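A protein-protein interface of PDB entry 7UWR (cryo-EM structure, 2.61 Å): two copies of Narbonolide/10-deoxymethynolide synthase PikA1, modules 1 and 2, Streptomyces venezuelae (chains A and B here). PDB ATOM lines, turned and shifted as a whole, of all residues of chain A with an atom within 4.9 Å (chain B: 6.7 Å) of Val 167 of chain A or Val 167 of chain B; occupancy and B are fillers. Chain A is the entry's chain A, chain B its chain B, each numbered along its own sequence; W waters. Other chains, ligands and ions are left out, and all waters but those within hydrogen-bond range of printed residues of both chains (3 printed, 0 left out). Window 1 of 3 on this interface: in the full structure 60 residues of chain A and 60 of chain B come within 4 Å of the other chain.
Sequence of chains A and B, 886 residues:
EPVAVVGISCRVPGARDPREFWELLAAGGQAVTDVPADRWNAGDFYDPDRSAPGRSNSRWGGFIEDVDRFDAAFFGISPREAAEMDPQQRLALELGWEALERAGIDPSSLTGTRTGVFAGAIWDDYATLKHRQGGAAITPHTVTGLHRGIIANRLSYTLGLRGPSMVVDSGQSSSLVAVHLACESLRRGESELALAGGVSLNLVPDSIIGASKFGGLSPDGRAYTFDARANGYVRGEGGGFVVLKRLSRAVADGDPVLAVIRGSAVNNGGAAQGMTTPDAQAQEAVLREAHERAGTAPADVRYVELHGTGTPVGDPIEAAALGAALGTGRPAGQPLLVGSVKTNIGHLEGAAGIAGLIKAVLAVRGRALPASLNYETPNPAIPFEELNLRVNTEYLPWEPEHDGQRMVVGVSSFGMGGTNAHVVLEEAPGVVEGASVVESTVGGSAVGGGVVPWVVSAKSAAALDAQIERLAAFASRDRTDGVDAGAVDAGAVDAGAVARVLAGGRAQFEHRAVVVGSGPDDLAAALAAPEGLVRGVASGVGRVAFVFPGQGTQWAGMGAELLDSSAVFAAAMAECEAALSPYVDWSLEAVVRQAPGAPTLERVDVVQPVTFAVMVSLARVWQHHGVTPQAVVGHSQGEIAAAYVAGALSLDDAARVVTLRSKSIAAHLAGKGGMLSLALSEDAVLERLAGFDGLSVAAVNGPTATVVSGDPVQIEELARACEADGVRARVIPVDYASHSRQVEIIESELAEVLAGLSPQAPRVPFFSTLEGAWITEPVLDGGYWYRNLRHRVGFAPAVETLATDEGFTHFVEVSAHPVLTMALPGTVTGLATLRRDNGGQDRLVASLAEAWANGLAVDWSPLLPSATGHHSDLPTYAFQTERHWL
Water W1 bridges OD1 of Asp 169 of chain A (2.5 Å) and N of Gly 149 of chain B (3.3 Å). Water W3 lies within hydrogen-bond range of OD1 of Asp 169 of chain B (2.6 Å) and N of Gly 149 of chain A (3.3 Å). Water W2 lies within hydrogen-bond range of O of Val 167 of chain A, O of Val 167 of chain B, N of Asp 169 of chain B and N of Asp 169 of chain A.
Met 166 of chain A touches Asp 169 of chain B, and with the chains exchanged Asp 169 of chain A touches Met 166 of chain B. Val 167 of chain B touches its own counterpart, Val 167 of chain A. Val 167 of chain A touches Val 168 of chain B, and with the chains exchanged Val 168 of chain A touches Val 167 of chain B. Val 167 of chain A touches Asp 169 of chain B, and with the chains exchanged Asp 169 of chain A touches Val 167 of chain B. 12 positions are printed for both chains.
Printed residues of chain B within 4 Å of Gly 149 of chain A: Asp 169 (3.2 Å). Of the printed residues of chain A, Met 166 of chain B touches Val 168 (3.6 Å) and Asp 169 (3.9 Å). Val 167 of chain B touches just these residues of chain A: Val 167 (3.8 Å), Val 168 (3.5 Å) and Asp 169 (2.8 Å). The nearest residue of chain B that does not touch Val 167 of chain A is Ser 170 of chain B (5.0 Å). The nearest printed residue of chain A that does not touch Val 167 of chain B is Arg 148 of chain A (6.3 Å). The nearest printed residue of chain B that does not touch Ser 165 of chain A is Asp 169 of chain B (5.2 Å).
Hydrophobic or aromatic side chains of chain A within 4 Å of the printed part of chain B: Met 166, Val 167 and Val 168. Printed residues of chain B that touch a printed residue of chain A: Arg 148, Gly 149, Met 166, Val 167, Val 168, Asp 169 and Ser 170. Along chain B the printed residues that touch a printed residue of chain A span positions 148 to 170. Among the printed residues, no Asp or Glu carboxylate lies within 4 Å of a Lys or Arg side-chain nitrogen of the other chain.
Among the printed residues, pairs that only touch across the chains: Val 168 of chain A with Val 167 of chain B (3.5 Å), Val 167 of chain A with Val 168 of chain B (3.5 Å), Met 166 of chain A with Val 168 of chain B (3.6 Å), Val 168 of chain A with Met 166 of chain B (3.6 Å), Asp 169 of chain A with Arg 148 of chain B (3.7 Å), Arg 148 of chain A with Asp 169 of chain B (3.7 Å), Ser 165 of chain A with Ser 170 of chain B (3.8 Å), Val 167 of chain A with Val 167 of chain B (3.8 Å), Met 166 of chain A with Asp 169 of chain B (3.8 Å) and Asp 169 of chain A with Met 166 of chain B (3.9 Å).
The backbone NH (N) of Ala 121 of chain A lies within hydrogen-bond range of the backbone carbonyl oxygen (O) of Val 168 of chain A (3.3 Å). The backbone NH (N) of Val 168 of chain A is in hydrogen-bond range of the backbone carbonyl oxygen (O) of Ala 119 of chain A, 2.7 Å away. The backbone carbonyl oxygen (O) of Met 166 of chain B sits at hydrogen-bond distance from the backbone NH (N) of Ala 119 of chain B (3.2 Å). The side-chain amide nitrogen (ND2) of Asn 153 of chain B sits close to the backbone carbonyl oxygen (O) of Gly 149 of chain B (3.5 Å). The guanidinium group of Arg 148 of chain A lies within salt-bridge range of the side-chain carboxylate of Asp 169 of chain A (2.4 Å). The backbone carbonyl oxygen (O) of Ala 152 of chain A sits close to the side-chain hydroxyl (OG) of Ser 165 of chain A (3.3 Å).
The backbone NH (N) of Gly 149 of chain A sits at hydrogen-bond distance from the side-chain carboxylate (OD2) of Asp 169 of chain B (3.2 Å). O of Val 167 of chain A sits at hydrogen-bond distance from N of Asp 169 of chain B (2.8 Å). O of Val 167 of chain B sits at hydrogen-bond distance from N of Asp 169 of chain A, 2.8 Å away. The backbone NH of Gly 149 of chain B is in hydrogen-bond range of the side-chain carboxylate of Asp 169 of chain A, 3.2 Å away.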
ATOM      1  N   ALA A 119       4.924   1.108  -7.390  1.00  0.00           N
ATOM      2  CA  ALA A 119       4.274   2.160  -6.618  1.00  0.00           C
ATOM      3  C   ALA A 119       4.447   3.526  -7.269  1.00  0.00           C
ATOM      4  O   ALA A 119       5.541   3.870  -7.719  1.00  0.00           O
ATOM      5  CB  ALA A 119       4.826   2.197  -5.190  1.00  0.00           C
ATOM      6  N   GLY A 120       3.353   4.285  -7.340  1.00  0.00           N
ATOM      7  CA  GLY A 120       3.384   5.704  -7.643  1.00  0.00           C
ATOM      8  C   GLY A 120       3.525   6.569  -6.405  1.00  0.00           C
ATOM      9  O   GLY A 120       2.680   6.493  -5.510  1.00  0.00           O
ATOM     10  N   ALA A 121       4.565   7.399  -6.326  1.00  0.00           N
ATOM     11  CA  ALA A 121       4.679   8.382  -5.253  1.00  0.00           C
ATOM     12  C   ALA A 121       5.493   9.576  -5.732  1.00  0.00           C
ATOM     13  O   ALA A 121       6.450   9.412  -6.490  1.00  0.00           O
ATOM     14  CB  ALA A 121       5.328   7.771  -4.008  1.00  0.00           C
ATOM     15  N   ARG A 148      12.338   7.547  -2.095  1.00  0.00           N
ATOM     16  CA  ARG A 148      10.994   7.131  -2.482  1.00  0.00           C
ATOM     17  C   ARG A 148      10.955   5.729  -3.079  1.00  0.00           C
ATOM     18  O   ARG A 148       9.987   5.000  -2.861  1.00  0.00           O
ATOM     19  CB  ARG A 148      10.378   8.159  -3.428  1.00  0.00           C
ATOM     20  CG  ARG A 148       9.287   8.971  -2.743  1.00  0.00           C
ATOM     21  CD  ARG A 148       9.055  10.316  -3.393  1.00  0.00           C
ATOM     22  NE  ARG A 148       8.835  10.241  -4.829  1.00  0.00           N
ATOM     23  CZ  ARG A 148       9.010  11.260  -5.656  1.00  0.00           C
ATOM     24  NH1 ARG A 148       9.265  12.478  -5.206  1.00  0.00           N
ATOM     25  NH2 ARG A 148       8.891  11.063  -6.961  1.00  0.00           N
ATOM     26  N   GLY A 149      11.980   5.339  -3.834  1.00  0.00           N
ATOM     27  CA  GLY A 149      12.106   3.953  -4.263  1.00  0.00           C
ATOM     28  C   GLY A 149      12.057   2.924  -3.147  1.00  0.00           C
ATOM     29  O   GLY A 149      11.550   1.814  -3.345  1.00  0.00           O
ATOM     30  N   ILE A 151       9.972   3.003  -0.792  1.00  0.00           N
ATOM     31  CA  ILE A 151       8.552   2.681  -0.645  1.00  0.00           C
ATOM     32  C   ILE A 151       8.242   1.357  -1.321  1.00  0.00           C
ATOM     33  O   ILE A 151       7.547   0.504  -0.760  1.00  0.00           O
ATOM     34  CB  ILE A 151       7.671   3.811  -1.212  1.00  0.00           C
ATOM     35  CG1 ILE A 151       7.904   5.126  -0.471  1.00  0.00           C
ATOM     36  CG2 ILE A 151       6.204   3.419  -1.176  1.00  0.00           C
ATOM     37  CD1 ILE A 151       7.306   6.323  -1.153  1.00  0.00           C
ATOM     38  N   ALA A 152       8.748   1.159  -2.531  1.00  0.00           N
ATOM     39  CA  ALA A 152       8.522  -0.139  -3.145  1.00  0.00           C
ATOM     40  C   ALA A 152       9.463  -1.190  -2.567  1.00  0.00           C
ATOM     41  O   ALA A 152       9.013  -2.259  -2.125  1.00  0.00           O
ATOM     42  CB  ALA A 152       8.680  -0.042  -4.662  1.00  0.00           C
ATOM     43  N   SER A 165      11.071  -4.127  -8.482  1.00  0.00           N
ATOM     44  CA  SER A 165      10.525  -3.239  -7.465  1.00  0.00           C
ATOM     45  C   SER A 165      11.006  -1.821  -7.718  1.00  0.00           C
ATOM     46  O   SER A 165      12.211  -1.560  -7.669  1.00  0.00           O
ATOM     47  CB  SER A 165      10.933  -3.705  -6.070  1.00  0.00           C
ATOM     48  OG  SER A 165      10.390  -2.872  -5.069  1.00  0.00           O
ATOM     49  N   MET A 166      10.072  -0.916  -7.983  1.00  0.00           N
ATOM     50  CA  MET A 166      10.433   0.453  -8.306  1.00  0.00           C
ATOM     51  C   MET A 166       9.257   1.357  -7.985  1.00  0.00           C
ATOM     52  O   MET A 166       8.100   0.931  -7.967  1.00  0.00           O
ATOM     53  CB  MET A 166      10.839   0.594  -9.776  1.00  0.00           C
ATOM     54  CG  MET A 166       9.700   0.383 -10.751  1.00  0.00           C
ATOM     55  SD  MET A 166      10.257  -0.232 -12.343  1.00  0.00           S
ATOM     56  CE  MET A 166      10.736  -1.897 -11.897  1.00  0.00           C
ATOM     57  N   VAL A 167       9.578   2.622  -7.750  1.00  0.00           N
ATOM     58  CA  VAL A 167       8.602   3.695  -7.648  1.00  0.00           C
ATOM     59  C   VAL A 167       8.622   4.506  -8.931  1.00  0.00           C
ATOM     60  O   VAL A 167       9.691   4.894  -9.417  1.00  0.00           O
ATOM     61  CB  VAL A 167       8.865   4.569  -6.412  1.00  0.00           C
ATOM     62  CG1 VAL A 167       7.928   5.757  -6.385  1.00  0.00           C
ATOM     63  CG2 VAL A 167       8.650   3.729  -5.182  1.00  0.00           C
ATOM     64  N   VAL A 168       7.446   4.752  -9.483  1.00  0.00           N
ATOM     65  CA  VAL A 168       7.279   5.605 -10.650  1.00  0.00           C
ATOM     66  C   VAL A 168       6.763   6.962 -10.198  1.00  0.00           C
ATOM     67  O   VAL A 168       5.896   7.058  -9.320  1.00  0.00           O
ATOM     68  CB  VAL A 168       6.351   4.950 -11.693  1.00  0.00           C
ATOM     69  CG1 VAL A 168       4.913   4.914 -11.216  1.00  0.00           C
ATOM     70  CG2 VAL A 168       6.449   5.684 -13.019  1.00  0.00           C
ATOM     71  N   ASP A 169       7.338   8.017 -10.763  1.00  0.00           N
ATOM     72  CA  ASP A 169       6.827   9.371 -10.604  1.00  0.00           C
ATOM     73  C   ASP A 169       6.528   9.918 -11.991  1.00  0.00           C
ATOM     74  O   ASP A 169       7.445  10.252 -12.749  1.00  0.00           O
ATOM     75  CB  ASP A 169       7.832  10.239  -9.847  1.00  0.00           C
ATOM     76  CG  ASP A 169       7.312  11.635  -9.548  1.00  0.00           C
ATOM     77  OD1 ASP A 169       6.212  11.992 -10.012  1.00  0.00           O
ATOM     78  OD2 ASP A 169       8.002  12.372  -8.814  1.00  0.00           O
ATOM     79  N   VAL B 117      10.231   8.869 -22.780  1.00  0.00           N
ATOM     80  CA  VAL B 117      11.297   9.334 -21.895  1.00  0.00           C
ATOM     81  C   VAL B 117      11.263   8.524 -20.608  1.00  0.00           C
ATOM     82  O   VAL B 117      10.245   8.500 -19.906  1.00  0.00           O
ATOM     83  CB  VAL B 117      11.181  10.835 -21.596  1.00  0.00           C
ATOM     84  CG1 VAL B 117      12.382  11.297 -20.798  1.00  0.00           C
ATOM     85  CG2 VAL B 117      11.078  11.611 -22.879  1.00  0.00           C
ATOM     86  N   PHE B 118      12.378   7.860 -20.308  1.00  0.00           N
ATOM     87  CA  PHE B 118      12.523   6.989 -19.142  1.00  0.00           C
ATOM     88  C   PHE B 118      13.773   7.437 -18.389  1.00  0.00           C
ATOM     89  O   PHE B 118      14.893   7.137 -18.809  1.00  0.00           O
ATOM     90  CB  PHE B 118      12.625   5.534 -19.573  1.00  0.00           C
ATOM     91  CG  PHE B 118      11.430   5.041 -20.326  1.00  0.00           C
ATOM     92  CD1 PHE B 118      10.355   4.482 -19.659  1.00  0.00           C
ATOM     93  CD2 PHE B 118      11.373   5.151 -21.706  1.00  0.00           C
ATOM     94  CE1 PHE B 118       9.258   4.026 -20.352  1.00  0.00           C
ATOM     95  CE2 PHE B 118      10.277   4.698 -22.403  1.00  0.00           C
ATOM     96  CZ  PHE B 118       9.217   4.135 -21.725  1.00  0.00           C
ATOM     97  N   ALA B 119      13.594   8.151 -17.280  1.00  0.00           N
ATOM     98  CA  ALA B 119      14.708   8.689 -16.509  1.00  0.00           C
ATOM     99  C   ALA B 119      14.761   8.098 -15.106  1.00  0.00           C
ATOM    100  O   ALA B 119      13.731   7.978 -14.439  1.00  0.00           O
ATOM    101  CB  ALA B 119      14.612  10.215 -16.421  1.00  0.00           C
ATOM    102  N   GLY B 120      15.961   7.705 -14.680  1.00  0.00           N
ATOM    103  CA  GLY B 120      16.256   7.406 -13.290  1.00  0.00           C
ATOM    104  C   GLY B 120      16.722   8.622 -12.511  1.00  0.00           C
ATOM    105  O   GLY B 120      17.724   9.236 -12.884  1.00  0.00           O
ATOM    106  N   ALA B 121      16.030   8.986 -11.431  1.00  0.00           N
ATOM    107  CA  ALA B 121      16.508  10.034 -10.535  1.00  0.00           C
ATOM    108  C   ALA B 121      15.973   9.795  -9.130  1.00  0.00           C
ATOM    109  O   ALA B 121      14.836   9.347  -8.966  1.00  0.00           O
ATOM    110  CB  ALA B 121      16.086  11.421 -11.028  1.00  0.00           C
ATOM    111  N   ILE B 122      16.791  10.101  -8.119  1.00  0.00           N
ATOM    112  CA  ILE B 122      16.530   9.610  -6.766  1.00  0.00           C
ATOM    113  C   ILE B 122      16.849  10.658  -5.705  1.00  0.00           C
ATOM    114  O   ILE B 122      16.247  10.653  -4.625  1.00  0.00           O
ATOM    115  CB  ILE B 122      17.310   8.308  -6.464  1.00  0.00           C
ATOM    116  CG1 ILE B 122      18.777   8.595  -6.153  1.00  0.00           C
ATOM    117  CG2 ILE B 122      17.215   7.305  -7.605  1.00  0.00           C
ATOM    118  CD1 ILE B 122      19.605   7.356  -5.941  1.00  0.00           C
ATOM    119  N   HIS B 147       9.505  18.645  -8.651  1.00  0.00           N
ATOM    120  CA  HIS B 147       8.957  17.304  -8.808  1.00  0.00           C
ATOM    121  C   HIS B 147       9.796  16.508  -9.800  1.00  0.00           C
ATOM    122  O   HIS B 147      10.132  16.995 -10.881  1.00  0.00           O
ATOM    123  CB  HIS B 147       7.502  17.374  -9.259  1.00  0.00           C
ATOM    124  CG  HIS B 147       6.522  17.205  -8.143  1.00  0.00           C
ATOM    125  ND1 HIS B 147       6.355  18.141  -7.144  1.00  0.00           N
ATOM    126  CD2 HIS B 147       5.653  16.204  -7.867  1.00  0.00           C
ATOM    127  CE1 HIS B 147       5.429  17.721  -6.301  1.00  0.00           C
ATOM    128  NE2 HIS B 147       4.987  16.549  -6.718  1.00  0.00           N
ATOM    129  N   ARG B 148      10.136  15.276  -9.424  1.00  0.00           N
ATOM    130  CA  ARG B 148      11.138  14.523 -10.169  1.00  0.00           C
ATOM    131  C   ARG B 148      10.603  13.958 -11.480  1.00  0.00           C
ATOM    132  O   ARG B 148      11.342  13.896 -12.464  1.00  0.00           O
ATOM    133  CB  ARG B 148      11.733  13.427  -9.289  1.00  0.00           C
ATOM    134  CG  ARG B 148      13.158  13.757  -8.865  1.00  0.00           C
ATOM    135  CD  ARG B 148      13.576  13.052  -7.595  1.00  0.00           C
ATOM    136  NE  ARG B 148      13.354  11.615  -7.626  1.00  0.00           N
ATOM    137  CZ  ARG B 148      13.257  10.860  -6.542  1.00  0.00           C
ATOM    138  NH1 ARG B 148      13.499  11.349  -5.336  1.00  0.00           N
ATOM    139  NH2 ARG B 148      12.943   9.579  -6.671  1.00  0.00           N
ATOM    140  N   GLY B 149       9.342  13.536 -11.513  1.00  0.00           N
ATOM    141  CA  GLY B 149       8.708  13.178 -12.776  1.00  0.00           C
ATOM    142  C   GLY B 149       8.769  14.246 -13.854  1.00  0.00           C
ATOM    143  O   GLY B 149       8.859  13.925 -15.045  1.00  0.00           O
ATOM    144  N   ILE B 150       8.832  15.518 -13.458  1.00  0.00           N
ATOM    145  CA  ILE B 150       9.008  16.593 -14.427  1.00  0.00           C
ATOM    146  C   ILE B 150      10.350  16.527 -15.138  1.00  0.00           C
ATOM    147  O   ILE B 150      10.424  16.900 -16.316  1.00  0.00           O
ATOM    148  CB  ILE B 150       8.836  17.961 -13.736  1.00  0.00           C
ATOM    149  CG1 ILE B 150       7.532  18.006 -12.938  1.00  0.00           C
ATOM    150  CG2 ILE B 150       8.871  19.091 -14.745  1.00  0.00           C
ATOM    151  CD1 ILE B 150       6.304  17.712 -13.759  1.00  0.00           C
ATOM    152  N   ILE B 151      11.360  15.899 -14.529  1.00  0.00           N
ATOM    153  CA  ILE B 151      12.609  15.634 -15.242  1.00  0.00           C
ATOM    154  C   ILE B 151      12.323  14.915 -16.550  1.00  0.00           C
ATOM    155  O   ILE B 151      12.872  15.262 -17.601  1.00  0.00           O
ATOM    156  CB  ILE B 151      13.583  14.823 -14.367  1.00  0.00           C
ATOM    157  CG1 ILE B 151      13.954  15.583 -13.094  1.00  0.00           C
ATOM    158  CG2 ILE B 151      14.823  14.440 -15.153  1.00  0.00           C
ATOM    159  CD1 ILE B 151      14.656  14.743 -12.067  1.00  0.00           C
ATOM    160  N   ALA B 152      11.465  13.906 -16.511  1.00  0.00           N
ATOM    161  CA  ALA B 152      11.126  13.268 -17.773  1.00  0.00           C
ATOM    162  C   ALA B 152      10.124  14.106 -18.559  1.00  0.00           C
ATOM    163  O   ALA B 152      10.353  14.413 -19.740  1.00  0.00           O
ATOM    164  CB  ALA B 152      10.585  11.860 -17.529  1.00  0.00           C
ATOM    165  N   ASN B 153       9.114  14.641 -17.870  1.00  0.00           N
ATOM    166  CA  ASN B 153       7.989  15.252 -18.570  1.00  0.00           C
ATOM    167  C   ASN B 153       8.386  16.541 -19.264  1.00  0.00           C
ATOM    168  O   ASN B 153       7.981  16.784 -20.407  1.00  0.00           O
ATOM    169  CB  ASN B 153       6.839  15.502 -17.596  1.00  0.00           C
ATOM    170  CG  ASN B 153       6.241  14.219 -17.044  1.00  0.00           C
ATOM    171  OD1 ASN B 153       5.385  14.253 -16.164  1.00  0.00           O
ATOM    172  ND2 ASN B 153       6.666  13.082 -17.584  1.00  0.00           N
ATOM    173  N   SER B 165       6.152   8.943 -20.501  1.00  0.00           N
ATOM    174  CA  SER B 165       7.192   9.748 -19.876  1.00  0.00           C
ATOM    175  C   SER B 165       7.088   9.627 -18.366  1.00  0.00           C
ATOM    176  O   SER B 165       6.075  10.018 -17.783  1.00  0.00           O
ATOM    177  CB  SER B 165       7.074  11.207 -20.308  1.00  0.00           C
ATOM    178  OG  SER B 165       8.092  11.999 -19.733  1.00  0.00           O
ATOM    179  N   MET B 166       8.130   9.092 -17.740  1.00  0.00           N
ATOM    180  CA  MET B 166       8.103   8.869 -16.306  1.00  0.00           C
ATOM    181  C   MET B 166       9.531   8.827 -15.790  1.00  0.00           C
ATOM    182  O   MET B 166      10.473   8.516 -16.523  1.00  0.00           O
ATOM    183  CB  MET B 166       7.361   7.578 -15.952  1.00  0.00           C
ATOM    184  CG  MET B 166       8.071   6.319 -16.402  1.00  0.00           C
ATOM    185  SD  MET B 166       6.938   4.963 -16.723  1.00  0.00           S
ATOM    186  CE  MET B 166       6.146   5.549 -18.215  1.00  0.00           C
ATOM    187  N   VAL B 167       9.666   9.128 -14.507  1.00  0.00           N
ATOM    188  CA  VAL B 167      10.897   8.931 -13.758  1.00  0.00           C
ATOM    189  C   VAL B 167      10.753   7.698 -12.884  1.00  0.00           C
ATOM    190  O   VAL B 167       9.750   7.536 -12.180  1.00  0.00           O
ATOM    191  CB  VAL B 167      11.253  10.179 -12.937  1.00  0.00           C
ATOM    192  CG1 VAL B 167      12.460   9.919 -12.061  1.00  0.00           C
ATOM    193  CG2 VAL B 167      11.552  11.305 -13.888  1.00  0.00           C
ATOM    194  N   VAL B 168      11.747   6.827 -12.937  1.00  0.00           N
ATOM    195  CA  VAL B 168      11.818   5.651 -12.084  1.00  0.00           C
ATOM    196  C   VAL B 168      12.809   5.918 -10.962  1.00  0.00           C
ATOM    197  O   VAL B 168      13.876   6.507 -11.173  1.00  0.00           O
ATOM    198  CB  VAL B 168      12.189   4.393 -12.897  1.00  0.00           C
ATOM    199  CG1 VAL B 168      13.630   4.436 -13.366  1.00  0.00           C
ATOM    200  CG2 VAL B 168      11.939   3.142 -12.071  1.00  0.00           C
ATOM    201  N   ASP B 169      12.427   5.529  -9.750  1.00  0.00           N
ATOM    202  CA  ASP B 169      13.330   5.517  -8.607  1.00  0.00           C
ATOM    203  C   ASP B 169      13.373   4.096  -8.067  1.00  0.00           C
ATOM    204  O   ASP B 169      12.417   3.630  -7.438  1.00  0.00           O
ATOM    205  CB  ASP B 169      12.869   6.520  -7.549  1.00  0.00           C
ATOM    206  CG  ASP B 169      13.832   6.639  -6.379  1.00  0.00           C
ATOM    207  OD1 ASP B 169      14.813   5.874  -6.311  1.00  0.00           O
ATOM    208  OD2 ASP B 169      13.616   7.531  -5.533  1.00  0.00           O
ATOM    209  N   SER B 170      14.486   3.419  -8.328  1.00  0.00           N
ATOM    210  CA  SER B 170      14.893   2.178  -7.684  1.00  0.00           C
ATOM    211  C   SER B 170      16.291   2.331  -7.103  1.00  0.00           C
ATOM    212  O   SER B 170      17.085   1.388  -7.106  1.00  0.00           O
ATOM    213  CB  SER B 170      14.830   1.005  -8.662  1.00  0.00           C
ATOM    214  OG  SER B 170      15.857   1.100  -9.626  1.00  0.00           O
ATOM    215  N   LEU B 181      13.090  -0.462 -18.764  1.00  0.00           N
ATOM    216  CA  LEU B 181      11.721  -0.073 -19.082  1.00  0.00           C
ATOM    217  C   LEU B 181      11.598   0.442 -20.506  1.00  0.00           C
ATOM    218  O   LEU B 181      10.746  -0.032 -21.270  1.00  0.00           O
ATOM    219  CB  LEU B 181      11.227   0.985 -18.096  1.00  0.00           C
ATOM    220  CG  LEU B 181      10.980   0.553 -16.653  1.00  0.00           C
ATOM    221  CD1 LEU B 181      10.637   1.759 -15.807  1.00  0.00           C
ATOM    222  CD2 LEU B 181       9.874  -0.483 -16.589  1.00  0.00           C
HETATM  223  O   HOH W   1       6.259  14.365 -10.871  1.00  0.00           O
HETATM  224  O   HOH W   2      10.204   7.854  -9.184  1.00  0.00           O
HETATM  225  O   HOH W   3      15.242   4.995  -3.906  1.00  0.00           O
